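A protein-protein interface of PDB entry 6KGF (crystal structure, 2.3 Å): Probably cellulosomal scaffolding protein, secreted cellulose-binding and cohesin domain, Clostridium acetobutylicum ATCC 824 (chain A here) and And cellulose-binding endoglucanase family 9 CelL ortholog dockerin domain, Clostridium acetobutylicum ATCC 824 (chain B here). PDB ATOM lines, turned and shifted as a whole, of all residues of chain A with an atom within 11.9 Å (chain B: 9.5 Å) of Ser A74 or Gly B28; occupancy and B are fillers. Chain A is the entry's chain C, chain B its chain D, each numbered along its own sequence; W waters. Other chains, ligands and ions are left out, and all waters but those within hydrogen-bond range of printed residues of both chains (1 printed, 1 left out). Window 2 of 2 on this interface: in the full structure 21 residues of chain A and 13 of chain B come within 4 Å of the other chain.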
ATOM      1  N   MET A  40      -9.533  20.146  -6.261  1.00  0.00           N
ATOM      2  CA  MET A  40      -8.096  20.228  -6.469  1.00  0.00           C
ATOM      3  C   MET A  40      -7.812  20.739  -7.871  1.00  0.00           C
ATOM      4  O   MET A  40      -8.560  20.465  -8.814  1.00  0.00           O
ATOM      5  CB  MET A  40      -7.417  18.869  -6.261  1.00  0.00           C
ATOM      6  CG  MET A  40      -7.754  17.824  -7.311  1.00  0.00           C
ATOM      7  SD  MET A  40      -6.891  16.265  -7.024  1.00  0.00           S
ATOM      8  CE  MET A  40      -5.180  16.795  -7.112  1.00  0.00           C
ATOM      9  N   ASP A  41      -6.720  21.490  -7.992  1.00  0.00           N
ATOM     10  CA  ASP A  41      -6.227  21.982  -9.269  1.00  0.00           C
ATOM     11  C   ASP A  41      -4.852  21.386  -9.529  1.00  0.00           C
ATOM     12  O   ASP A  41      -4.032  21.268  -8.612  1.00  0.00           O
ATOM     13  CB  ASP A  41      -6.151  23.511  -9.282  1.00  0.00           C
ATOM     14  CG  ASP A  41      -7.503  24.161  -9.073  1.00  0.00           C
ATOM     15  OD1 ASP A  41      -8.508  23.615  -9.573  1.00  0.00           O
ATOM     16  OD2 ASP A  41      -7.560  25.216  -8.407  1.00  0.00           O
ATOM     17  N   ILE A  42      -4.606  21.000 -10.778  1.00  0.00           N
ATOM     18  CA  ILE A  42      -3.328  20.437 -11.193  1.00  0.00           C
ATOM     19  C   ILE A  42      -2.785  21.304 -12.318  1.00  0.00           C
ATOM     20  O   ILE A  42      -3.451  21.486 -13.346  1.00  0.00           O
ATOM     21  CB  ILE A  42      -3.456  18.973 -11.639  1.00  0.00           C
ATOM     22  CG1 ILE A  42      -4.063  18.130 -10.515  1.00  0.00           C
ATOM     23  CG2 ILE A  42      -2.084  18.421 -12.045  1.00  0.00           C
ATOM     24  CD1 ILE A  42      -4.533  16.757 -10.957  1.00  0.00           C
ATOM     25  N   SER A  43      -1.585  21.841 -12.121  1.00  0.00           N
ATOM     26  CA  SER A  43      -0.932  22.694 -13.102  1.00  0.00           C
ATOM     27  C   SER A  43       0.019  21.867 -13.957  1.00  0.00           C
ATOM     28  O   SER A  43       0.678  20.950 -13.461  1.00  0.00           O
ATOM     29  CB  SER A  43      -0.164  23.822 -12.410  1.00  0.00           C
ATOM     30  OG  SER A  43       0.541  24.610 -13.351  1.00  0.00           O
ATOM     31  N   TYR A  44       0.086  22.201 -15.245  1.00  0.00           N
ATOM     32  CA  TYR A  44       0.940  21.481 -16.178  1.00  0.00           C
ATOM     33  C   TYR A  44       1.461  22.455 -17.225  1.00  0.00           C
ATOM     34  O   TYR A  44       0.884  23.521 -17.456  1.00  0.00           O
ATOM     35  CB  TYR A  44       0.197  20.318 -16.851  1.00  0.00           C
ATOM     36  CG  TYR A  44      -0.955  20.747 -17.735  1.00  0.00           C
ATOM     37  CD1 TYR A  44      -2.223  20.943 -17.206  1.00  0.00           C
ATOM     38  CD2 TYR A  44      -0.775  20.955 -19.096  1.00  0.00           C
ATOM     39  CE1 TYR A  44      -3.281  21.335 -18.009  1.00  0.00           C
ATOM     40  CE2 TYR A  44      -1.829  21.348 -19.908  1.00  0.00           C
ATOM     41  CZ  TYR A  44      -3.078  21.537 -19.356  1.00  0.00           C
ATOM     42  OH  TYR A  44      -4.133  21.931 -20.152  1.00  0.00           O
ATOM     43  N   ALA A  46       1.702  23.798 -20.564  1.00  0.00           N
ATOM     44  CA  ALA A  46       0.852  23.728 -21.747  1.00  0.00           C
ATOM     45  C   ALA A  46       1.664  23.697 -23.036  1.00  0.00           C
ATOM     46  O   ALA A  46       1.202  23.143 -24.039  1.00  0.00           O
ATOM     47  CB  ALA A  46      -0.114  24.913 -21.769  1.00  0.00           C
ATOM     48  N   THR A  50      -0.787  18.425 -23.860  1.00  0.00           N
ATOM     49  CA  THR A  50      -2.188  18.734 -24.111  1.00  0.00           C
ATOM     50  C   THR A  50      -3.041  17.702 -23.389  1.00  0.00           C
ATOM     51  O   THR A  50      -2.850  16.494 -23.573  1.00  0.00           O
ATOM     52  CB  THR A  50      -2.499  18.731 -25.611  1.00  0.00           C
ATOM     53  OG1 THR A  50      -1.621  19.645 -26.285  1.00  0.00           O
ATOM     54  CG2 THR A  50      -3.945  19.142 -25.869  1.00  0.00           C
ATOM     55  N   VAL A  51      -3.969  18.177 -22.555  1.00  0.00           N
ATOM     56  CA  VAL A  51      -4.876  17.276 -21.854  1.00  0.00           C
ATOM     57  C   VAL A  51      -5.745  16.546 -22.866  1.00  0.00           C
ATOM     58  O   VAL A  51      -6.409  17.166 -23.704  1.00  0.00           O
ATOM     59  CB  VAL A  51      -5.733  18.057 -20.846  1.00  0.00           C
ATOM     60  CG1 VAL A  51      -6.815  17.161 -20.252  1.00  0.00           C
ATOM     61  CG2 VAL A  51      -4.854  18.633 -19.753  1.00  0.00           C
ATOM     62  N   LYS A  52      -5.739  15.217 -22.793  1.00  0.00           N
ATOM     63  CA  LYS A  52      -6.580  14.389 -23.647  1.00  0.00           C
ATOM     64  C   LYS A  52      -7.798  13.843 -22.917  1.00  0.00           C
ATOM     65  O   LYS A  52      -8.896  13.833 -23.481  1.00  0.00           O
ATOM     66  CB  LYS A  52      -5.771  13.221 -24.223  1.00  0.00           C
ATOM     67  CG  LYS A  52      -6.532  12.401 -25.255  1.00  0.00           C
ATOM     68  CD  LYS A  52      -5.760  11.164 -25.671  1.00  0.00           C
ATOM     69  CE  LYS A  52      -6.558  10.321 -26.652  1.00  0.00           C
ATOM     70  NZ  LYS A  52      -5.886   9.024 -26.941  1.00  0.00           N
ATOM     71  N   VAL A  54      -9.429  13.095 -18.603  1.00  0.00           N
ATOM     72  CA  VAL A  54      -9.340  13.084 -17.148  1.00  0.00           C
ATOM     73  C   VAL A  54     -10.507  12.231 -16.676  1.00  0.00           C
ATOM     74  O   VAL A  54     -11.647  12.706 -16.611  1.00  0.00           O
ATOM     75  CB  VAL A  54      -9.403  14.498 -16.545  1.00  0.00           C
ATOM     76  CG1 VAL A  54      -9.308  14.434 -15.022  1.00  0.00           C
ATOM     77  CG2 VAL A  54      -8.308  15.372 -17.124  1.00  0.00           C
ATOM     78  N   TYR A  67     -23.008  12.703 -12.025  1.00  0.00           N
ATOM     79  CA  TYR A  67     -22.064  13.820 -12.086  1.00  0.00           C
ATOM     80  C   TYR A  67     -21.388  14.059 -10.734  1.00  0.00           C
ATOM     81  O   TYR A  67     -21.313  15.187 -10.246  1.00  0.00           O
ATOM     82  CB  TYR A  67     -22.758  15.095 -12.575  1.00  0.00           C
ATOM     83  CG  TYR A  67     -23.521  14.930 -13.871  1.00  0.00           C
ATOM     84  CD1 TYR A  67     -24.843  14.507 -13.871  1.00  0.00           C
ATOM     85  CD2 TYR A  67     -22.921  15.206 -15.092  1.00  0.00           C
ATOM     86  CE1 TYR A  67     -25.545  14.356 -15.051  1.00  0.00           C
ATOM     87  CE2 TYR A  67     -23.616  15.058 -16.277  1.00  0.00           C
ATOM     88  CZ  TYR A  67     -24.928  14.632 -16.250  1.00  0.00           C
ATOM     89  OH  TYR A  67     -25.629  14.483 -17.426  1.00  0.00           O
ATOM     90  N   PHE A  69     -18.195  13.374 -10.434  1.00  0.00           N
ATOM     91  CA  PHE A  69     -16.824  13.690 -10.827  1.00  0.00           C
ATOM     92  C   PHE A  69     -16.884  14.705 -11.960  1.00  0.00           C
ATOM     93  O   PHE A  69     -17.283  14.368 -13.080  1.00  0.00           O
ATOM     94  CB  PHE A  69     -16.085  12.422 -11.254  1.00  0.00           C
ATOM     95  CG  PHE A  69     -14.620  12.626 -11.526  1.00  0.00           C
ATOM     96  CD1 PHE A  69     -13.708  12.689 -10.485  1.00  0.00           C
ATOM     97  CD2 PHE A  69     -14.151  12.730 -12.825  1.00  0.00           C
ATOM     98  CE1 PHE A  69     -12.358  12.866 -10.735  1.00  0.00           C
ATOM     99  CE2 PHE A  69     -12.804  12.907 -13.080  1.00  0.00           C
ATOM    100  CZ  PHE A  69     -11.906  12.976 -12.033  1.00  0.00           C
ATOM    101  N   ILE A  70     -16.492  15.943 -11.671  1.00  0.00           N
ATOM    102  CA  ILE A  70     -16.543  17.038 -12.634  1.00  0.00           C
ATOM    103  C   ILE A  70     -15.120  17.455 -12.977  1.00  0.00           C
ATOM    104  O   ILE A  70     -14.275  17.608 -12.084  1.00  0.00           O
ATOM    105  CB  ILE A  70     -17.352  18.227 -12.088  1.00  0.00           C
ATOM    106  CG1 ILE A  70     -18.820  17.823 -11.925  1.00  0.00           C
ATOM    107  CG2 ILE A  70     -17.224  19.427 -13.012  1.00  0.00           C
ATOM    108  CD1 ILE A  70     -19.678  18.846 -11.199  1.00  0.00           C
ATOM    109  N   VAL A  71     -14.860  17.648 -14.267  1.00  0.00           N
ATOM    110  CA  VAL A  71     -13.555  18.065 -14.763  1.00  0.00           C
ATOM    111  C   VAL A  71     -13.714  19.403 -15.467  1.00  0.00           C
ATOM    112  O   VAL A  71     -14.683  19.619 -16.202  1.00  0.00           O
ATOM    113  CB  VAL A  71     -12.946  17.020 -15.721  1.00  0.00           C
ATOM    114  CG1 VAL A  71     -11.589  17.488 -16.230  1.00  0.00           C
ATOM    115  CG2 VAL A  71     -12.821  15.671 -15.025  1.00  0.00           C
ATOM    116  N   ASN A  72     -12.761  20.301 -15.237  1.00  0.00           N
ATOM    117  CA  ASN A  72     -12.724  21.590 -15.914  1.00  0.00           C
ATOM    118  C   ASN A  72     -11.320  21.826 -16.446  1.00  0.00           C
ATOM    119  O   ASN A  72     -10.345  21.767 -15.688  1.00  0.00           O
ATOM    120  CB  ASN A  72     -13.134  22.728 -14.976  1.00  0.00           C
ATOM    121  CG  ASN A  72     -13.096  24.082 -15.654  1.00  0.00           C
ATOM    122  OD1 ASN A  72     -12.031  24.565 -16.044  1.00  0.00           O
ATOM    123  ND2 ASN A  72     -14.258  24.706 -15.796  1.00  0.00           N
ATOM    124  N   THR A  73     -11.223  22.089 -17.749  1.00  0.00           N
ATOM    125  CA  THR A  73      -9.955  22.393 -18.402  1.00  0.00           C
ATOM    126  C   THR A  73     -10.048  23.708 -19.164  1.00  0.00           C
ATOM    127  O   THR A  73      -9.308  23.932 -20.127  1.00  0.00           O
ATOM    128  CB  THR A  73      -9.537  21.261 -19.340  1.00  0.00           C
ATOM    129  OG1 THR A  73     -10.503  21.121 -20.387  1.00  0.00           O
ATOM    130  CG2 THR A  73      -9.435  19.949 -18.584  1.00  0.00           C
ATOM    131  N   SER A  74     -10.957  24.591 -18.743  1.00  0.00           N
ATOM    132  CA  SER A  74     -11.154  25.861 -19.427  1.00  0.00           C
ATOM    133  C   SER A  74      -9.969  26.804 -19.268  1.00  0.00           C
ATOM    134  O   SER A  74      -9.885  27.796 -20.002  1.00  0.00           O
ATOM    135  CB  SER A  74     -12.421  26.544 -18.907  1.00  0.00           C
ATOM    136  OG  SER A  74     -13.563  25.727 -19.105  1.00  0.00           O
ATOM    137  N   THR A  75      -9.057  26.525 -18.321  1.00  0.00           N
ATOM    138  CA  THR A  75      -7.898  27.385 -18.106  1.00  0.00           C
ATOM    139  C   THR A  75      -6.663  26.751 -18.720  1.00  0.00           C
ATOM    140  O   THR A  75      -6.421  25.554 -18.502  1.00  0.00           O
ATOM    141  CB  THR A  75      -7.668  27.615 -16.615  1.00  0.00           C
ATOM    142  OG1 THR A  75      -8.877  28.087 -16.008  1.00  0.00           O
ATOM    143  CG2 THR A  75      -6.559  28.643 -16.392  1.00  0.00           C
ATOM    144  N   PRO A  76      -5.856  27.490 -19.481  1.00  0.00           N
ATOM    145  CA  PRO A  76      -4.638  26.889 -20.039  1.00  0.00           C
ATOM    146  C   PRO A  76      -3.717  26.402 -18.931  1.00  0.00           C
ATOM    147  O   PRO A  76      -3.411  27.134 -17.987  1.00  0.00           O
ATOM    148  CB  PRO A  76      -4.000  28.033 -20.838  1.00  0.00           C
ATOM    149  CG  PRO A  76      -5.047  29.071 -20.985  1.00  0.00           C
ATOM    150  CD  PRO A  76      -5.980  28.917 -19.826  1.00  0.00           C
ATOM    151  N   GLY A  77      -3.285  25.150 -19.047  1.00  0.00           N
ATOM    152  CA  GLY A  77      -2.312  24.613 -18.118  1.00  0.00           C
ATOM    153  C   GLY A  77      -2.843  24.289 -16.743  1.00  0.00           C
ATOM    154  O   GLY A  77      -2.056  24.182 -15.800  1.00  0.00           O
ATOM    155  N   LYS A  78      -4.156  24.118 -16.596  1.00  0.00           N
ATOM    156  CA  LYS A  78      -4.747  23.811 -15.302  1.00  0.00           C
ATOM    157  C   LYS A  78      -5.898  22.834 -15.480  1.00  0.00           C
ATOM    158  O   LYS A  78      -6.736  23.007 -16.370  1.00  0.00           O
ATOM    159  CB  LYS A  78      -5.243  25.082 -14.595  1.00  0.00           C
ATOM    160  CG  LYS A  78      -5.905  24.818 -13.243  1.00  0.00           C
ATOM    161  CD  LYS A  78      -6.085  26.095 -12.426  1.00  0.00           C
ATOM    162  CE  LYS A  78      -7.153  27.012 -13.013  1.00  0.00           C
ATOM    163  NZ  LYS A  78      -8.523  26.423 -12.946  1.00  0.00           N
ATOM    164  N   ILE A  79      -5.925  21.811 -14.630  1.00  0.00           N
ATOM    165  CA  ILE A  79      -7.015  20.846 -14.565  1.00  0.00           C
ATOM    166  C   ILE A  79      -7.661  20.988 -13.196  1.00  0.00           C
ATOM    167  O   ILE A  79      -6.986  20.833 -12.170  1.00  0.00           O
ATOM    168  CB  ILE A  79      -6.524  19.406 -14.776  1.00  0.00           C
ATOM    169  CG1 ILE A  79      -5.801  19.267 -16.116  1.00  0.00           C
ATOM    170  CG2 ILE A  79      -7.699  18.429 -14.695  1.00  0.00           C
ATOM    171  CD1 ILE A  79      -4.998  17.984 -16.233  1.00  0.00           C
ATOM    172  N   SER A  80      -8.959  21.274 -13.175  1.00  0.00           N
ATOM    173  CA  SER A  80      -9.719  21.377 -11.936  1.00  0.00           C
ATOM    174  C   SER A  80     -10.589  20.135 -11.800  1.00  0.00           C
ATOM    175  O   SER A  80     -11.417  19.855 -12.675  1.00  0.00           O
ATOM    176  CB  SER A  80     -10.576  22.643 -11.913  1.00  0.00           C
ATOM    177  OG  SER A  80      -9.771  23.808 -11.951  1.00  0.00           O
ATOM    178  N   ILE A  81     -10.385  19.389 -10.719  1.00  0.00           N
ATOM    179  CA  ILE A  81     -11.145  18.181 -10.426  1.00  0.00           C
ATOM    180  C   ILE A  81     -12.018  18.453  -9.211  1.00  0.00           C
ATOM    181  O   ILE A  81     -11.519  18.889  -8.165  1.00  0.00           O
ATOM    182  CB  ILE A  81     -10.220  16.976 -10.178  1.00  0.00           C
ATOM    183  CG1 ILE A  81      -9.422  16.656 -11.445  1.00  0.00           C
ATOM    184  CG2 ILE A  81     -11.028  15.763  -9.728  1.00  0.00           C
ATOM    185  CD1 ILE A  81      -8.378  15.579 -11.260  1.00  0.00           C
ATOM    186  N   THR A  82     -13.317  18.196  -9.347  1.00  0.00           N
ATOM    187  CA  THR A  82     -14.271  18.331  -8.253  1.00  0.00           C
ATOM    188  C   THR A  82     -14.984  17.001  -8.059  1.00  0.00           C
ATOM    189  O   THR A  82     -15.655  16.515  -8.976  1.00  0.00           O
ATOM    190  CB  THR A  82     -15.290  19.439  -8.541  1.00  0.00           C
ATOM    191  OG1 THR A  82     -14.610  20.678  -8.758  1.00  0.00           O
ATOM    192  CG2 THR A  82     -16.257  19.596  -7.377  1.00  0.00           C
ATOM    193  N   VAL B  20     -28.219  21.274 -11.515  1.00  0.00           N
ATOM    194  CA  VAL B  20     -27.771  21.021 -12.883  1.00  0.00           C
ATOM    195  C   VAL B  20     -26.934  22.189 -13.389  1.00  0.00           C
ATOM    196  O   VAL B  20     -25.863  22.000 -13.979  1.00  0.00           O
ATOM    197  CB  VAL B  20     -28.976  20.752 -13.803  1.00  0.00           C
ATOM    198  CG1 VAL B  20     -28.554  20.794 -15.265  1.00  0.00           C
ATOM    199  CG2 VAL B  20     -29.611  19.408 -13.471  1.00  0.00           C
ATOM    200  N   MET B  21     -27.413  23.415 -13.167  1.00  0.00           N
ATOM    201  CA  MET B  21     -26.685  24.592 -13.630  1.00  0.00           C
ATOM    202  C   MET B  21     -25.316  24.686 -12.965  1.00  0.00           C
ATOM    203  O   MET B  21     -24.302  24.913 -13.636  1.00  0.00           O
ATOM    204  CB  MET B  21     -27.506  25.853 -13.358  1.00  0.00           C
ATOM    205  CG  MET B  21     -28.678  26.044 -14.307  1.00  0.00           C
ATOM    206  SD  MET B  21     -29.392  27.700 -14.221  1.00  0.00           S
ATOM    207  CE  MET B  21     -30.469  27.671 -15.651  1.00  0.00           C
ATOM    208  N   MET B  22     -25.269  24.516 -11.641  1.00  0.00           N
ATOM    209  CA  MET B  22     -23.997  24.565 -10.930  1.00  0.00           C
ATOM    210  C   MET B  22     -23.022  23.536 -11.488  1.00  0.00           C
ATOM    211  O   MET B  22     -21.852  23.844 -11.741  1.00  0.00           O
ATOM    212  CB  MET B  22     -24.227  24.330  -9.436  1.00  0.00           C
ATOM    213  CG  MET B  22     -22.953  24.321  -8.607  1.00  0.00           C
ATOM    214  SD  MET B  22     -22.179  25.946  -8.522  1.00  0.00           S
ATOM    215  CE  MET B  22     -23.216  26.752  -7.300  1.00  0.00           C
ATOM    216  N   ARG B  23     -23.490  22.301 -11.681  1.00  0.00           N
ATOM    217  CA  ARG B  23     -22.629  21.260 -12.226  1.00  0.00           C
ATOM    218  C   ARG B  23     -22.123  21.642 -13.610  1.00  0.00           C
ATOM    219  O   ARG B  23     -20.924  21.547 -13.894  1.00  0.00           O
ATOM    220  CB  ARG B  23     -23.384  19.932 -12.276  1.00  0.00           C
ATOM    221  CG  ARG B  23     -23.591  19.283 -10.926  1.00  0.00           C
ATOM    222  CD  ARG B  23     -24.499  18.069 -11.045  1.00  0.00           C
ATOM    223  NE  ARG B  23     -24.714  17.423  -9.756  1.00  0.00           N
ATOM    224  CZ  ARG B  23     -25.618  16.475  -9.533  1.00  0.00           C
ATOM    225  NH1 ARG B  23     -26.404  16.053 -10.516  1.00  0.00           N
ATOM    226  NH2 ARG B  23     -25.737  15.951  -8.322  1.00  0.00           N
ATOM    227  N   GLN B  24     -23.028  22.089 -14.485  1.00  0.00           N
ATOM    228  CA  GLN B  24     -22.636  22.455 -15.842  1.00  0.00           C
ATOM    229  C   GLN B  24     -21.682  23.642 -15.841  1.00  0.00           C
ATOM    230  O   GLN B  24     -20.753  23.702 -16.658  1.00  0.00           O
ATOM    231  CB  GLN B  24     -23.879  22.769 -16.677  1.00  0.00           C
ATOM    232  CG  GLN B  24     -24.765  21.562 -16.939  1.00  0.00           C
ATOM    233  CD  GLN B  24     -26.006  21.900 -17.743  1.00  0.00           C
ATOM    234  OE1 GLN B  24     -26.441  23.051 -17.785  1.00  0.00           O
ATOM    235  NE2 GLN B  24     -26.584  20.892 -18.386  1.00  0.00           N
ATOM    236  N   TYR B  25     -21.895  24.602 -14.937  1.00  0.00           N
ATOM    237  CA  TYR B  25     -21.004  25.754 -14.864  1.00  0.00           C
ATOM    238  C   TYR B  25     -19.617  25.349 -14.376  1.00  0.00           C
ATOM    239  O   TYR B  25     -18.605  25.834 -14.896  1.00  0.00           O
ATOM    240  CB  TYR B  25     -21.595  26.822 -13.946  1.00  0.00           C
ATOM    241  CG  TYR B  25     -20.698  28.029 -13.786  1.00  0.00           C
ATOM    242  CD1 TYR B  25     -20.781  29.103 -14.663  1.00  0.00           C
ATOM    243  CD2 TYR B  25     -19.762  28.092 -12.764  1.00  0.00           C
ATOM    244  CE1 TYR B  25     -19.961  30.206 -14.523  1.00  0.00           C
ATOM    245  CE2 TYR B  25     -18.936  29.189 -12.616  1.00  0.00           C
ATOM    246  CZ  TYR B  25     -19.039  30.242 -13.498  1.00  0.00           C
ATOM    247  OH  TYR B  25     -18.216  31.336 -13.351  1.00  0.00           O
ATOM    248  N   LEU B  26     -19.552  24.468 -13.375  1.00  0.00           N
ATOM    249  CA  LEU B  26     -18.265  24.035 -12.846  1.00  0.00           C
ATOM    250  C   LEU B  26     -17.456  23.267 -13.883  1.00  0.00           C
ATOM    251  O   LEU B  26     -16.221  23.269 -13.827  1.00  0.00           O
ATOM    252  CB  LEU B  26     -18.476  23.180 -11.597  1.00  0.00           C
ATOM    253  CG  LEU B  26     -18.761  23.940 -10.300  1.00  0.00           C
ATOM    254  CD1 LEU B  26     -19.125  22.970  -9.190  1.00  0.00           C
ATOM    255  CD2 LEU B  26     -17.558  24.796  -9.895  1.00  0.00           C
ATOM    256  N   ALA B  27     -18.125  22.604 -14.827  1.00  0.00           N
ATOM    257  CA  ALA B  27     -17.445  21.907 -15.911  1.00  0.00           C
ATOM    258  C   ALA B  27     -16.998  22.843 -17.025  1.00  0.00           C
ATOM    259  O   ALA B  27     -16.388  22.378 -17.996  1.00  0.00           O
ATOM    260  CB  ALA B  27     -18.357  20.825 -16.497  1.00  0.00           C
ATOM    261  N   GLY B  28     -17.289  24.136 -16.918  1.00  0.00           N
ATOM    262  CA  GLY B  28     -16.901  25.087 -17.936  1.00  0.00           C
ATOM    263  C   GLY B  28     -17.858  25.207 -19.096  1.00  0.00           C
ATOM    264  O   GLY B  28     -17.496  25.803 -20.117  1.00  0.00           O
ATOM    265  N   LYS B  29     -19.063  24.655 -18.981  1.00  0.00           N
ATOM    266  CA  LYS B  29     -20.054  24.773 -20.037  1.00  0.00           C
ATOM    267  C   LYS B  29     -20.763  26.118 -19.946  1.00  0.00           C
ATOM    268  O   LYS B  29     -20.870  26.719 -18.874  1.00  0.00           O
ATOM    269  CB  LYS B  29     -21.077  23.641 -19.945  1.00  0.00           C
ATOM    270  CG  LYS B  29     -20.482  22.250 -20.093  1.00  0.00           C
ATOM    271  CD  LYS B  29     -21.527  21.176 -19.837  1.00  0.00           C
ATOM    272  CE  LYS B  29     -20.930  19.783 -19.948  1.00  0.00           C
ATOM    273  NZ  LYS B  29     -21.927  18.724 -19.616  1.00  0.00           N
ATOM    274  N   THR B  30     -21.242  26.592 -21.092  1.00  0.00           N
ATOM    275  CA  THR B  30     -22.036  27.814 -21.145  1.00  0.00           C
ATOM    276  C   THR B  30     -23.467  27.463 -20.754  1.00  0.00           C
ATOM    277  O   THR B  30     -24.147  26.715 -21.464  1.00  0.00           O
ATOM    278  CB  THR B  30     -21.975  28.439 -22.534  1.00  0.00           C
ATOM    279  OG1 THR B  30     -20.606  28.633 -22.911  1.00  0.00           O
ATOM    280  CG2 THR B  30     -22.692  29.783 -22.552  1.00  0.00           C
ATOM    281  N   VAL B  31     -23.917  27.991 -19.621  1.00  0.00           N
ATOM    282  CA  VAL B  31     -25.233  27.687 -19.072  1.00  0.00           C
ATOM    283  C   VAL B  31     -26.158  28.850 -19.404  1.00  0.00           C
ATOM    284  O   VAL B  31     -26.005  29.951 -18.865  1.00  0.00           O
ATOM    285  CB  VAL B  31     -25.169  27.444 -17.559  1.00  0.00           C
ATOM    286  CG1 VAL B  31     -26.517  26.959 -17.039  1.00  0.00           C
ATOM    287  CG2 VAL B  31     -24.069  26.449 -17.229  1.00  0.00           C
ATOM    288  N   VAL B  47     -16.099  30.452  -6.758  1.00  0.00           N
ATOM    289  CA  VAL B  47     -17.136  29.526  -7.202  1.00  0.00           C
ATOM    290  C   VAL B  47     -16.445  28.200  -7.482  1.00  0.00           C
ATOM    291  O   VAL B  47     -15.698  28.078  -8.464  1.00  0.00           O
ATOM    292  CB  VAL B  47     -17.879  30.037  -8.444  1.00  0.00           C
ATOM    293  CG1 VAL B  47     -18.997  29.075  -8.835  1.00  0.00           C
ATOM    294  CG2 VAL B  47     -18.438  31.426  -8.190  1.00  0.00           C
HETATM  295  O   HOH W   1     -13.702  22.661 -19.043  1.00  0.00           O
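ND2 of Asn A72 lies close to N of Gly B28, 3.3 Å away.
ND2 of Asn A72 is in hydrogen-bond range of O of Leu B26 (3.1 Å).
The side-chain amide oxygen of Asn A72 lies within hydrogen-bond range of the backbone NH of Ser A74 (2.9 Å).
N of Ser A80 sits at hydrogen-bond distance from O of Asn A72 (2.9 Å).
O of Thr A82 is in hydrogen-bond range of N of Ile A70 (2.9 Å).
Among the printed residues, merely in contact across the chains: Tyr A67 with Arg B23, Ile A70 with Arg B23, Ile A70 with Leu B26, Ile A70 with Ala B27, Val A71 with Ala B27, Asn A72 with Ala B27 and Ser A74 with Gly B28.
Ser A43 touches none of the printed residues of chain B.
Thr A50 touches none of the printed residues of chain B.
Of the printed residues of chain B, Val A71 touches Ala B27.
Of the printed residues of chain B, Asn A72 touches Leu B26 (3.1 Å), Ala B27 (3.5 Å) and Gly B28 (3.3 Å).
No residue of chain B comes within 4 Å of Thr A73.
Of chain B, only Gly B28 (3.6 Å) comes within 4 Å of Ser A74.
No residue of chain B comes within 4 Å of Thr A75.
Printed residues of chain A within 4 Å of Ala B27: Ile A70 (3.8 Å), Val A71 (3.6 Å) and Asn A72 (3.5 Å).
Gly B28 touches two residues of chain A.
No residue of chain A comes within 4 Å of Thr B30.
The nearest residue of chain B that does not touch Ser A74 is Ala B27 (4.5 Å).
The nearest residue of chain A that does not touch Gly B28 is Val A71 (5.3 Å).
The nearest printed residue of chain B that does not touch Asn A72 is Tyr B25 (4.6 Å).
Hydrophobic or aromatic side chains of chain A that line the printed part of chain B: Tyr A67 and Ile A70.
Of the 13 printed residues of chain B, 4 touch a printed residue of chain A.
Hydrophobic or aromatic side chains of chain B within 4 Å of the printed part of chain A: Ala B27.
Among the printed residues, no Asp or Glu carboxylate lies within 4 Å of a Lys or Arg side-chain nitrogen of the other chain.
Water W1 lies within hydrogen-bond range of the backbone NH of Thr A73, the backbone carbonyl oxygen of Ala B27 and the side-chain hydroxyl of Ser A74.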
